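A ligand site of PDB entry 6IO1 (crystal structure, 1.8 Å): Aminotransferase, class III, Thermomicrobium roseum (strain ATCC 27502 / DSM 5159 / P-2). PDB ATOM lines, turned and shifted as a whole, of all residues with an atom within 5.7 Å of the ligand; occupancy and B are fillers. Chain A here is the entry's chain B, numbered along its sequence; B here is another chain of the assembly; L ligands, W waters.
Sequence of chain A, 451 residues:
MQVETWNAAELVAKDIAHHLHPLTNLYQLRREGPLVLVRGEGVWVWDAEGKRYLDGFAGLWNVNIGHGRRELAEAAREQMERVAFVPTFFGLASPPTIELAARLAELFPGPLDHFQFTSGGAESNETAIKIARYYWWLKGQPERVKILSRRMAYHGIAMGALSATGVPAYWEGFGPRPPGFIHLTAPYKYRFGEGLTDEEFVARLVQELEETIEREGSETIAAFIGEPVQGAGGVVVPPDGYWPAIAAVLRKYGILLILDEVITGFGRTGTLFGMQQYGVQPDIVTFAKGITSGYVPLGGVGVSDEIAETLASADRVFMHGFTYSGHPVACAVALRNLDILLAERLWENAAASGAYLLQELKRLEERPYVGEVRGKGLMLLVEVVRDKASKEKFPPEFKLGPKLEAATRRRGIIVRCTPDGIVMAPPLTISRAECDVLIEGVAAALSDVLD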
ATOM      1  N   LEU A  60     -23.614 -31.991  -5.040  1.00  0.00           N
ATOM      2  CA  LEU A  60     -22.750 -30.953  -4.462  1.00  0.00           C
ATOM      3  C   LEU A  60     -21.623 -31.643  -3.679  1.00  0.00           C
ATOM      4  O   LEU A  60     -21.555 -31.569  -2.454  1.00  0.00           O
ATOM      5  CB  LEU A  60     -23.554 -30.003  -3.566  1.00  0.00           C
ATOM      6  CG  LEU A  60     -24.493 -29.055  -4.305  1.00  0.00           C
ATOM      7  CD1 LEU A  60     -25.239 -28.164  -3.327  1.00  0.00           C
ATOM      8  CD2 LEU A  60     -23.729 -28.211  -5.317  1.00  0.00           C
ATOM      9  N   TRP A  61     -20.741 -32.327  -4.409  1.00  0.00           N
ATOM     10  CA  TRP A  61     -19.634 -33.107  -3.861  1.00  0.00           C
ATOM     11  C   TRP A  61     -20.099 -34.208  -2.909  1.00  0.00           C
ATOM     12  O   TRP A  61     -19.297 -34.702  -2.105  1.00  0.00           O
ATOM     13  CB  TRP A  61     -18.605 -32.241  -3.103  1.00  0.00           C
ATOM     14  CG  TRP A  61     -18.286 -30.867  -3.634  1.00  0.00           C
ATOM     15  CD1 TRP A  61     -19.086 -29.757  -3.578  1.00  0.00           C
ATOM     16  CD2 TRP A  61     -17.046 -30.441  -4.207  1.00  0.00           C
ATOM     17  NE1 TRP A  61     -18.429 -28.684  -4.114  1.00  0.00           N
ATOM     18  CE2 TRP A  61     -17.178 -29.064  -4.513  1.00  0.00           C
ATOM     19  CE3 TRP A  61     -15.839 -31.079  -4.521  1.00  0.00           C
ATOM     20  CZ2 TRP A  61     -16.152 -28.334  -5.116  1.00  0.00           C
ATOM     21  CZ3 TRP A  61     -14.829 -30.352  -5.119  1.00  0.00           C
ATOM     22  CH2 TRP A  61     -14.994 -28.995  -5.403  1.00  0.00           C
ATOM     23  N   SER A 119     -27.215 -30.935  10.530  1.00  0.00           N
ATOM     24  CA  SER A 119     -27.847 -31.196   9.237  1.00  0.00           C
ATOM     25  C   SER A 119     -27.048 -30.681   8.042  1.00  0.00           C
ATOM     26  O   SER A 119     -27.492 -30.855   6.911  1.00  0.00           O
ATOM     27  CB  SER A 119     -29.250 -30.598   9.207  1.00  0.00           C
ATOM     28  OG  SER A 119     -30.109 -31.255  10.123  1.00  0.00           O
ATOM     29  N   GLY A 120     -25.883 -30.063   8.270  1.00  0.00           N
ATOM     30  CA  GLY A 120     -25.141 -29.526   7.142  1.00  0.00           C
ATOM     31  C   GLY A 120     -23.744 -29.094   7.540  1.00  0.00           C
ATOM     32  O   GLY A 120     -23.388 -29.075   8.719  1.00  0.00           O
ATOM     33  N   GLY A 121     -22.963 -28.749   6.521  1.00  0.00           N
ATOM     34  CA  GLY A 121     -21.584 -28.337   6.746  1.00  0.00           C
ATOM     35  C   GLY A 121     -21.455 -27.044   7.519  1.00  0.00           C
ATOM     36  O   GLY A 121     -20.607 -26.923   8.400  1.00  0.00           O
ATOM     37  N   ALA A 122     -22.278 -26.042   7.171  1.00  0.00           N
ATOM     38  CA  ALA A 122     -22.220 -24.769   7.891  1.00  0.00           C
ATOM     39  C   ALA A 122     -22.593 -24.958   9.360  1.00  0.00           C
ATOM     40  O   ALA A 122     -21.964 -24.370  10.238  1.00  0.00           O
ATOM     41  CB  ALA A 122     -23.136 -23.743   7.231  1.00  0.00           C
ATOM     42  N   GLU A 123     -23.627 -25.756   9.626  1.00  0.00           N
ATOM     43  CA  GLU A 123     -23.983 -26.058  11.008  1.00  0.00           C
ATOM     44  C   GLU A 123     -22.821 -26.723  11.728  1.00  0.00           C
ATOM     45  O   GLU A 123     -22.517 -26.389  12.886  1.00  0.00           O
ATOM     46  CB  GLU A 123     -25.214 -26.973  11.047  1.00  0.00           C
ATOM     47  CG  GLU A 123     -26.542 -26.276  10.788  1.00  0.00           C
ATOM     48  CD  GLU A 123     -27.721 -27.201  10.990  1.00  0.00           C
ATOM     49  OE1 GLU A 123     -27.507 -28.379  11.360  1.00  0.00           O
ATOM     50  OE2 GLU A 123     -28.872 -26.757  10.791  1.00  0.00           O
ATOM     51  N   ASN A 125     -19.511 -26.513  11.051  1.00  0.00           N
ATOM     52  CA  ASN A 125     -18.412 -25.589  11.285  1.00  0.00           C
ATOM     53  C   ASN A 125     -18.767 -24.569  12.372  1.00  0.00           C
ATOM     54  O   ASN A 125     -17.899 -24.216  13.193  1.00  0.00           O
ATOM     55  CB  ASN A 125     -18.028 -24.896   9.979  1.00  0.00           C
ATOM     56  CG  ASN A 125     -17.231 -25.805   9.070  1.00  0.00           C
ATOM     57  OD1 ASN A 125     -16.518 -26.692   9.527  1.00  0.00           O
ATOM     58  ND2 ASN A 125     -17.353 -25.600   7.760  1.00  0.00           N
ATOM     59  N   TYR A 154     -13.597 -22.189   2.108  1.00  0.00           N
ATOM     60  CA  TYR A 154     -15.052 -22.167   2.135  1.00  0.00           C
ATOM     61  C   TYR A 154     -15.539 -23.115   3.224  1.00  0.00           C
ATOM     62  O   TYR A 154     -15.325 -24.334   3.134  1.00  0.00           O
ATOM     63  CB  TYR A 154     -15.655 -22.551   0.779  1.00  0.00           C
ATOM     64  CG  TYR A 154     -17.159 -22.398   0.757  1.00  0.00           C
ATOM     65  CD1 TYR A 154     -17.748 -21.164   0.521  1.00  0.00           C
ATOM     66  CD2 TYR A 154     -17.985 -23.486   0.989  1.00  0.00           C
ATOM     67  CE1 TYR A 154     -19.119 -21.022   0.520  1.00  0.00           C
ATOM     68  CE2 TYR A 154     -19.357 -23.353   0.977  1.00  0.00           C
ATOM     69  CZ  TYR A 154     -19.923 -22.121   0.737  1.00  0.00           C
ATOM     70  OH  TYR A 154     -21.295 -21.988   0.725  1.00  0.00           O
ATOM     71  N   HIS A 155     -16.186 -22.569   4.249  1.00  0.00           N
ATOM     72  CA  HIS A 155     -16.660 -23.357   5.383  1.00  0.00           C
ATOM     73  C   HIS A 155     -18.156 -23.193   5.625  1.00  0.00           C
ATOM     74  O   HIS A 155     -18.660 -23.655   6.659  1.00  0.00           O
ATOM     75  CB  HIS A 155     -15.890 -22.972   6.643  1.00  0.00           C
ATOM     76  CG  HIS A 155     -14.398 -23.104   6.515  1.00  0.00           C
ATOM     77  ND1 HIS A 155     -13.768 -24.326   6.460  1.00  0.00           N
ATOM     78  CD2 HIS A 155     -13.434 -22.167   6.434  1.00  0.00           C
ATOM     79  CE1 HIS A 155     -12.468 -24.138   6.339  1.00  0.00           C
ATOM     80  NE2 HIS A 155     -12.235 -22.833   6.317  1.00  0.00           N
ATOM     81  N   GLY A 156     -18.884 -22.584   4.706  1.00  0.00           N
ATOM     82  CA  GLY A 156     -20.298 -22.292   4.867  1.00  0.00           C
ATOM     83  C   GLY A 156     -20.577 -20.802   4.818  1.00  0.00           C
ATOM     84  O   GLY A 156     -19.679 -19.964   4.937  1.00  0.00           O
ATOM     85  N   ILE A 157     -21.855 -20.486   4.643  1.00  0.00           N
ATOM     86  CA  ILE A 157     -22.260 -19.093   4.493  1.00  0.00           C
ATOM     87  C   ILE A 157     -23.194 -18.641   5.608  1.00  0.00           C
ATOM     88  O   ILE A 157     -23.851 -17.609   5.490  1.00  0.00           O
ATOM     89  CB  ILE A 157     -22.892 -18.860   3.108  1.00  0.00           C
ATOM     90  CG1 ILE A 157     -23.766 -20.046   2.687  1.00  0.00           C
ATOM     91  CG2 ILE A 157     -21.811 -18.637   2.059  1.00  0.00           C
ATOM     92  CD1 ILE A 157     -25.106 -20.111   3.401  1.00  0.00           C
ATOM     93  N   GLU A 227      -9.726 -26.858   5.314  1.00  0.00           N
ATOM     94  CA  GLU A 227      -9.978 -28.083   4.564  1.00  0.00           C
ATOM     95  C   GLU A 227      -8.653 -28.716   4.161  1.00  0.00           C
ATOM     96  O   GLU A 227      -7.689 -28.011   3.853  1.00  0.00           O
ATOM     97  CB  GLU A 227     -10.788 -27.779   3.300  1.00  0.00           C
ATOM     98  CG  GLU A 227     -12.025 -26.923   3.527  1.00  0.00           C
ATOM     99  CD  GLU A 227     -12.373 -26.077   2.315  1.00  0.00           C
ATOM    100  OE1 GLU A 227     -12.985 -26.616   1.367  1.00  0.00           O
ATOM    101  OE2 GLU A 227     -12.048 -24.873   2.302  1.00  0.00           O
ATOM    102  N   ALA A 232     -14.491 -25.590  -2.673  1.00  0.00           N
ATOM    103  CA  ALA A 232     -15.225 -24.538  -3.349  1.00  0.00           C
ATOM    104  C   ALA A 232     -14.310 -23.379  -3.754  1.00  0.00           C
ATOM    105  O   ALA A 232     -14.581 -22.707  -4.750  1.00  0.00           O
ATOM    106  CB  ALA A 232     -16.367 -24.032  -2.468  1.00  0.00           C
ATOM    107  N   ASP A 260     -11.792 -29.414   8.326  1.00  0.00           N
ATOM    108  CA  ASP A 260     -13.087 -29.402   7.648  1.00  0.00           C
ATOM    109  C   ASP A 260     -13.056 -30.509   6.597  1.00  0.00           C
ATOM    110  O   ASP A 260     -12.507 -30.333   5.508  1.00  0.00           O
ATOM    111  CB  ASP A 260     -13.347 -28.030   7.041  1.00  0.00           C
ATOM    112  CG  ASP A 260     -14.705 -27.924   6.363  1.00  0.00           C
ATOM    113  OD1 ASP A 260     -15.306 -28.967   6.025  1.00  0.00           O
ATOM    114  OD2 ASP A 260     -15.171 -26.790   6.157  1.00  0.00           O
ATOM    115  N   VAL A 262     -15.834 -31.799   5.216  1.00  0.00           N
ATOM    116  CA  VAL A 262     -17.176 -31.847   4.640  1.00  0.00           C
ATOM    117  C   VAL A 262     -17.136 -32.395   3.216  1.00  0.00           C
ATOM    118  O   VAL A 262     -17.969 -33.213   2.822  1.00  0.00           O
ATOM    119  CB  VAL A 262     -17.829 -30.462   4.706  1.00  0.00           C
ATOM    120  CG1 VAL A 262     -19.042 -30.388   3.781  1.00  0.00           C
ATOM    121  CG2 VAL A 262     -18.240 -30.145   6.144  1.00  0.00           C
ATOM    122  N   ILE A 263     -16.152 -31.960   2.427  1.00  0.00           N
ATOM    123  CA  ILE A 263     -16.006 -32.450   1.055  1.00  0.00           C
ATOM    124  C   ILE A 263     -15.079 -33.654   0.988  1.00  0.00           C
ATOM    125  O   ILE A 263     -15.419 -34.681   0.406  1.00  0.00           O
ATOM    126  CB  ILE A 263     -15.505 -31.316   0.134  1.00  0.00           C
ATOM    127  CG1 ILE A 263     -16.587 -30.258  -0.064  1.00  0.00           C
ATOM    128  CG2 ILE A 263     -15.061 -31.878  -1.205  1.00  0.00           C
ATOM    129  CD1 ILE A 263     -16.189 -29.182  -1.047  1.00  0.00           C
ATOM    130  N   ALA A 288     -19.890 -33.677   6.600  1.00  0.00           N
ATOM    131  CA  ALA A 288     -21.223 -33.556   6.024  1.00  0.00           C
ATOM    132  C   ALA A 288     -21.215 -34.236   4.665  1.00  0.00           C
ATOM    133  O   ALA A 288     -20.313 -35.015   4.373  1.00  0.00           O
ATOM    134  CB  ALA A 288     -21.640 -32.090   5.900  1.00  0.00           C
ATOM    135  N   LYS A 289     -22.230 -33.955   3.840  1.00  0.00           N
ATOM    136  CA  LYS A 289     -22.244 -34.408   2.460  1.00  0.00           C
ATOM    137  C   LYS A 289     -22.205 -35.932   2.351  1.00  0.00           C
ATOM    138  O   LYS A 289     -23.233 -36.604   2.544  1.00  0.00           O
ATOM    139  CB  LYS A 289     -21.058 -33.802   1.689  1.00  0.00           C
ATOM    140  CG  LYS A 289     -21.147 -32.304   1.489  1.00  0.00           C
ATOM    141  CD  LYS A 289     -20.080 -31.807   0.526  1.00  0.00           C
ATOM    142  CE  LYS A 289     -20.192 -30.311   0.277  1.00  0.00           C
ATOM    143  NZ  LYS A 289     -21.518 -29.921  -0.249  1.00  0.00           N
ATOM    144  N   PHE B  89     -28.861 -25.393  -6.319  1.00  0.00           N
ATOM    145  CA  PHE B  89     -27.808 -24.505  -6.769  1.00  0.00           C
ATOM    146  C   PHE B  89     -27.770 -24.463  -8.288  1.00  0.00           C
ATOM    147  O   PHE B  89     -28.264 -25.360  -8.972  1.00  0.00           O
ATOM    148  CB  PHE B  89     -26.442 -24.965  -6.240  1.00  0.00           C
ATOM    149  CG  PHE B  89     -26.220 -24.717  -4.771  1.00  0.00           C
ATOM    150  CD1 PHE B  89     -27.244 -24.857  -3.852  1.00  0.00           C
ATOM    151  CD2 PHE B  89     -24.955 -24.369  -4.319  1.00  0.00           C
ATOM    152  CE1 PHE B  89     -27.022 -24.635  -2.508  1.00  0.00           C
ATOM    153  CE2 PHE B  89     -24.728 -24.139  -2.973  1.00  0.00           C
ATOM    154  CZ  PHE B  89     -25.758 -24.274  -2.067  1.00  0.00           C
ATOM    155  N   GLU B 123     -31.020 -22.069  10.188  1.00  0.00           N
ATOM    156  CA  GLU B 123     -30.651 -21.764   8.810  1.00  0.00           C
ATOM    157  C   GLU B 123     -31.661 -20.816   8.175  1.00  0.00           C
ATOM    158  O   GLU B 123     -31.277 -19.872   7.472  1.00  0.00           O
ATOM    159  CB  GLU B 123     -30.554 -23.053   7.992  1.00  0.00           C
ATOM    160  CG  GLU B 123     -29.309 -23.887   8.238  1.00  0.00           C
ATOM    161  CD  GLU B 123     -29.203 -25.067   7.306  1.00  0.00           C
ATOM    162  OE1 GLU B 123     -30.074 -25.209   6.418  1.00  0.00           O
ATOM    163  OE2 GLU B 123     -28.245 -25.868   7.441  1.00  0.00           O
ATOM    164  N   GLY B 321     -26.538 -19.819   0.088  1.00  0.00           N
ATOM    165  CA  GLY B 321     -27.190 -21.103  -0.032  1.00  0.00           C
ATOM    166  C   GLY B 321     -26.586 -22.190   0.825  1.00  0.00           C
ATOM    167  O   GLY B 321     -25.374 -22.258   1.006  1.00  0.00           O
ATOM    168  N   PHE B 322     -27.446 -23.050   1.346  1.00  0.00           N
ATOM    169  CA  PHE B 322     -27.026 -24.243   2.073  1.00  0.00           C
ATOM    170  C   PHE B 322     -27.095 -25.441   1.150  1.00  0.00           C
ATOM    171  O   PHE B 322     -27.947 -25.513   0.266  1.00  0.00           O
ATOM    172  CB  PHE B 322     -27.900 -24.466   3.313  1.00  0.00           C
ATOM    173  CG  PHE B 322     -27.812 -23.351   4.317  1.00  0.00           C
ATOM    174  CD1 PHE B 322     -26.804 -23.346   5.271  1.00  0.00           C
ATOM    175  CD2 PHE B 322     -28.721 -22.317   4.299  1.00  0.00           C
ATOM    176  CE1 PHE B 322     -26.725 -22.328   6.190  1.00  0.00           C
ATOM    177  CE2 PHE B 322     -28.638 -21.290   5.219  1.00  0.00           C
ATOM    178  CZ  PHE B 322     -27.643 -21.289   6.169  1.00  0.00           C
ATOM    179  N   THR B 323     -26.176 -26.396   1.369  1.00  0.00           N
ATOM    180  CA  THR B 323     -26.004 -27.497   0.425  1.00  0.00           C
ATOM    181  C   THR B 323     -27.316 -28.251   0.195  1.00  0.00           C
ATOM    182  O   THR B 323     -27.647 -28.582  -0.950  1.00  0.00           O
ATOM    183  CB  THR B 323     -24.928 -28.463   0.935  1.00  0.00           C
ATOM    184  OG1 THR B 323     -23.655 -27.807   0.903  1.00  0.00           O
ATOM    185  CG2 THR B 323     -24.876 -29.721   0.092  1.00  0.00           C
ATOM    186  N   TYR B 324     -28.073 -28.499   1.252  1.00  0.00           N
ATOM    187  CA  TYR B 324     -29.263 -29.336   1.166  1.00  0.00           C
ATOM    188  C   TYR B 324     -30.543 -28.522   0.952  1.00  0.00           C
ATOM    189  O   TYR B 324     -31.637 -29.028   1.215  1.00  0.00           O
ATOM    190  CB  TYR B 324     -29.375 -30.212   2.414  1.00  0.00           C
ATOM    191  CG  TYR B 324     -28.330 -31.306   2.392  1.00  0.00           C
ATOM    192  CD1 TYR B 324     -28.197 -32.124   1.284  1.00  0.00           C
ATOM    193  CD2 TYR B 324     -27.452 -31.489   3.455  1.00  0.00           C
ATOM    194  CE1 TYR B 324     -27.246 -33.111   1.231  1.00  0.00           C
ATOM    195  CE2 TYR B 324     -26.497 -32.481   3.414  1.00  0.00           C
ATOM    196  CZ  TYR B 324     -26.393 -33.292   2.297  1.00  0.00           C
ATOM    197  OH  TYR B 324     -25.442 -34.279   2.244  1.00  0.00           O
HETATM  198  N1  LIG L   1     -17.747 -26.855   4.504  1.00  0.00           N
HETATM  199  C1  LIG L   1     -17.265 -27.122   3.286  1.00  0.00           C
HETATM  200  C2  LIG L   1     -15.857 -27.638   3.159  1.00  0.00           C
HETATM  201  C3  LIG L   1     -18.047 -26.924   2.148  1.00  0.00           C
HETATM  202  O1  LIG L   1     -17.530 -27.197   0.921  1.00  0.00           O
HETATM  203  C4  LIG L   1     -19.355 -26.442   2.276  1.00  0.00           C
HETATM  204  C5  LIG L   1     -20.222 -26.219   1.069  1.00  0.00           C
HETATM  205  N2  LIG L   1     -19.889 -27.129  -0.038  1.00  0.00           N
HETATM  206  C6  LIG L   1     -19.845 -26.171   3.564  1.00  0.00           C
HETATM  207  C7  LIG L   1     -18.998 -26.397   4.640  1.00  0.00           C
HETATM  208  C8  LIG L   1     -21.239 -25.652   3.770  1.00  0.00           C
HETATM  209  O2  LIG L   1     -22.183 -26.753   3.923  1.00  0.00           O
HETATM  210  P1  LIG L   1     -23.772 -26.500   4.019  1.00  0.00           P
HETATM  211  O3  LIG L   1     -24.401 -27.869   4.191  1.00  0.00           O
HETATM  212  O4  LIG L   1     -23.966 -25.607   5.232  1.00  0.00           O
HETATM  213  O5  LIG L   1     -24.164 -25.825   2.722  1.00  0.00           O
HETATM  214  O   HOH W   1     -25.575 -26.276   7.454  1.00  0.00           O
HETATM  215  O   HOH W   2     -22.135 -29.069   2.991  1.00  0.00           O
HETATM  216  O   HOH W   3     -15.216 -25.826  -0.244  1.00  0.00           O
HETATM  217  O   HOH W   4     -23.034 -23.633   1.247  1.00  0.00           O
HETATM  218  O   HOH W   5     -26.873 -28.000   3.987  1.00  0.00           O
HETATM  219  O   HOH W   6     -23.293 -23.156   4.008  1.00  0.00           O
HETATM  220  O   HOH W   7     -22.447 -24.969  -0.874  1.00  0.00           O
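N of Tyr 154 is in hydrogen-bond range of OE2 of Glu 227 (3.1 Å).
OG1 of Thr 323 of chain B lies within hydrogen-bond range of NZ of Lys 289 (3.2 Å).
The backbone carbonyl oxygen of His 155 is in hydrogen-bond range of the side-chain amide nitrogen of Asn 125, at 2.6 Å.
The side-chain carboxylate of Asp 260 is in hydrogen-bond range of the side-chain amide nitrogen of Asn 125, at 3.0 Å.
The side-chain carboxylate (OD1) of Asp 260 is in hydrogen-bond range of the backbone NH (N) of Val 262 (3.0 Å).
O of Lys 289 sits close to OH of Tyr 324 of chain B (3.2 Å).
NZ of Lys 289 sits at hydrogen-bond distance from O of Leu 60 (2.8 Å).
The side-chain carboxylate of Asp 260 is in hydrogen-bond range of a ring nitrogen (ND1) of His 155 (2.9 Å).
OD2 of Asp 260 sits close to N1 of the ligand (3.1 Å).
CA of Gly 120 touches O3 of the ligand, at 3.5 Å.
Asn 125 touches the ligand (ND2 to N1, 3.5 Å).
CE2 of Tyr 154 touches C5 of the ligand, 3.0 Å away.
O of His 155 touches C7 of the ligand (3.4 Å).
CA of Gly 156 touches C8 of the ligand, at 3.7 Å.
Glu 227 touches the ligand.
Val 262 touches the ligand.
Ile 263 touches the ligand (CD1 to O1, 3.1 Å).
CA of Phe 322 of chain B touches O5 of the ligand (3.3 Å).
Of the 25 residues printed, 14 come within 4 Å of the ligand.
The nearest printed residue that does not touch the ligand is Gly 321 of chain B (4.1 Å).
Water W5 lies within hydrogen-bond range of O3 of the ligand (2.5 Å), N of Tyr 324 of chain B (3.0 Å) and N of Thr 323 of chain B (3.1 Å).
Water W2 lies within hydrogen-bond range of O2 of the ligand (2.5 Å), OG1 of Thr 323 of chain B (2.9 Å) and NZ of Lys 289 (3.4 Å).
Water W6 lies within hydrogen-bond range of O4 of the ligand (2.8 Å) and N of Ile 157 (3.1 Å).
Water W1 lies within hydrogen-bond range of the side-chain carboxylate (OE2) of Glu 123 of chain B (2.7 Å), an oxygen (O4) of the ligand (2.8 Å), the backbone NH (N) of Glu 123 of chain A (3.0 Å) and the backbone NH (N) of Ala 122 (3.3 Å).
Water W4 lies within hydrogen-bond range of the side-chain hydroxyl of Tyr 154, the backbone carbonyl oxygen of Gly 321 of chain B and an oxygen (O5) of the ligand.
Water W3 lies within hydrogen-bond range of N of Ala 232 (2.5 Å), OE1 of Glu 227 (2.9 Å) and O1 of the ligand (2.9 Å).
N2 of the ligand sits close to NZ of Lys 289 (3.2 Å).
The side-chain hydroxyl (OG1) of Thr 323 of chain B sits at hydrogen-bond distance from an oxygen (O5) of the ligand, 2.7 Å away.
N of Ala 122 lies within hydrogen-bond range of O4 of the ligand, 2.6 Å away.
An oxygen (O5) of the ligand sits at hydrogen-bond distance from the backbone NH of Thr 323 of chain B, 2.5 Å away.
N of Gly 121 sits at hydrogen-bond distance from O3 of the ligand.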
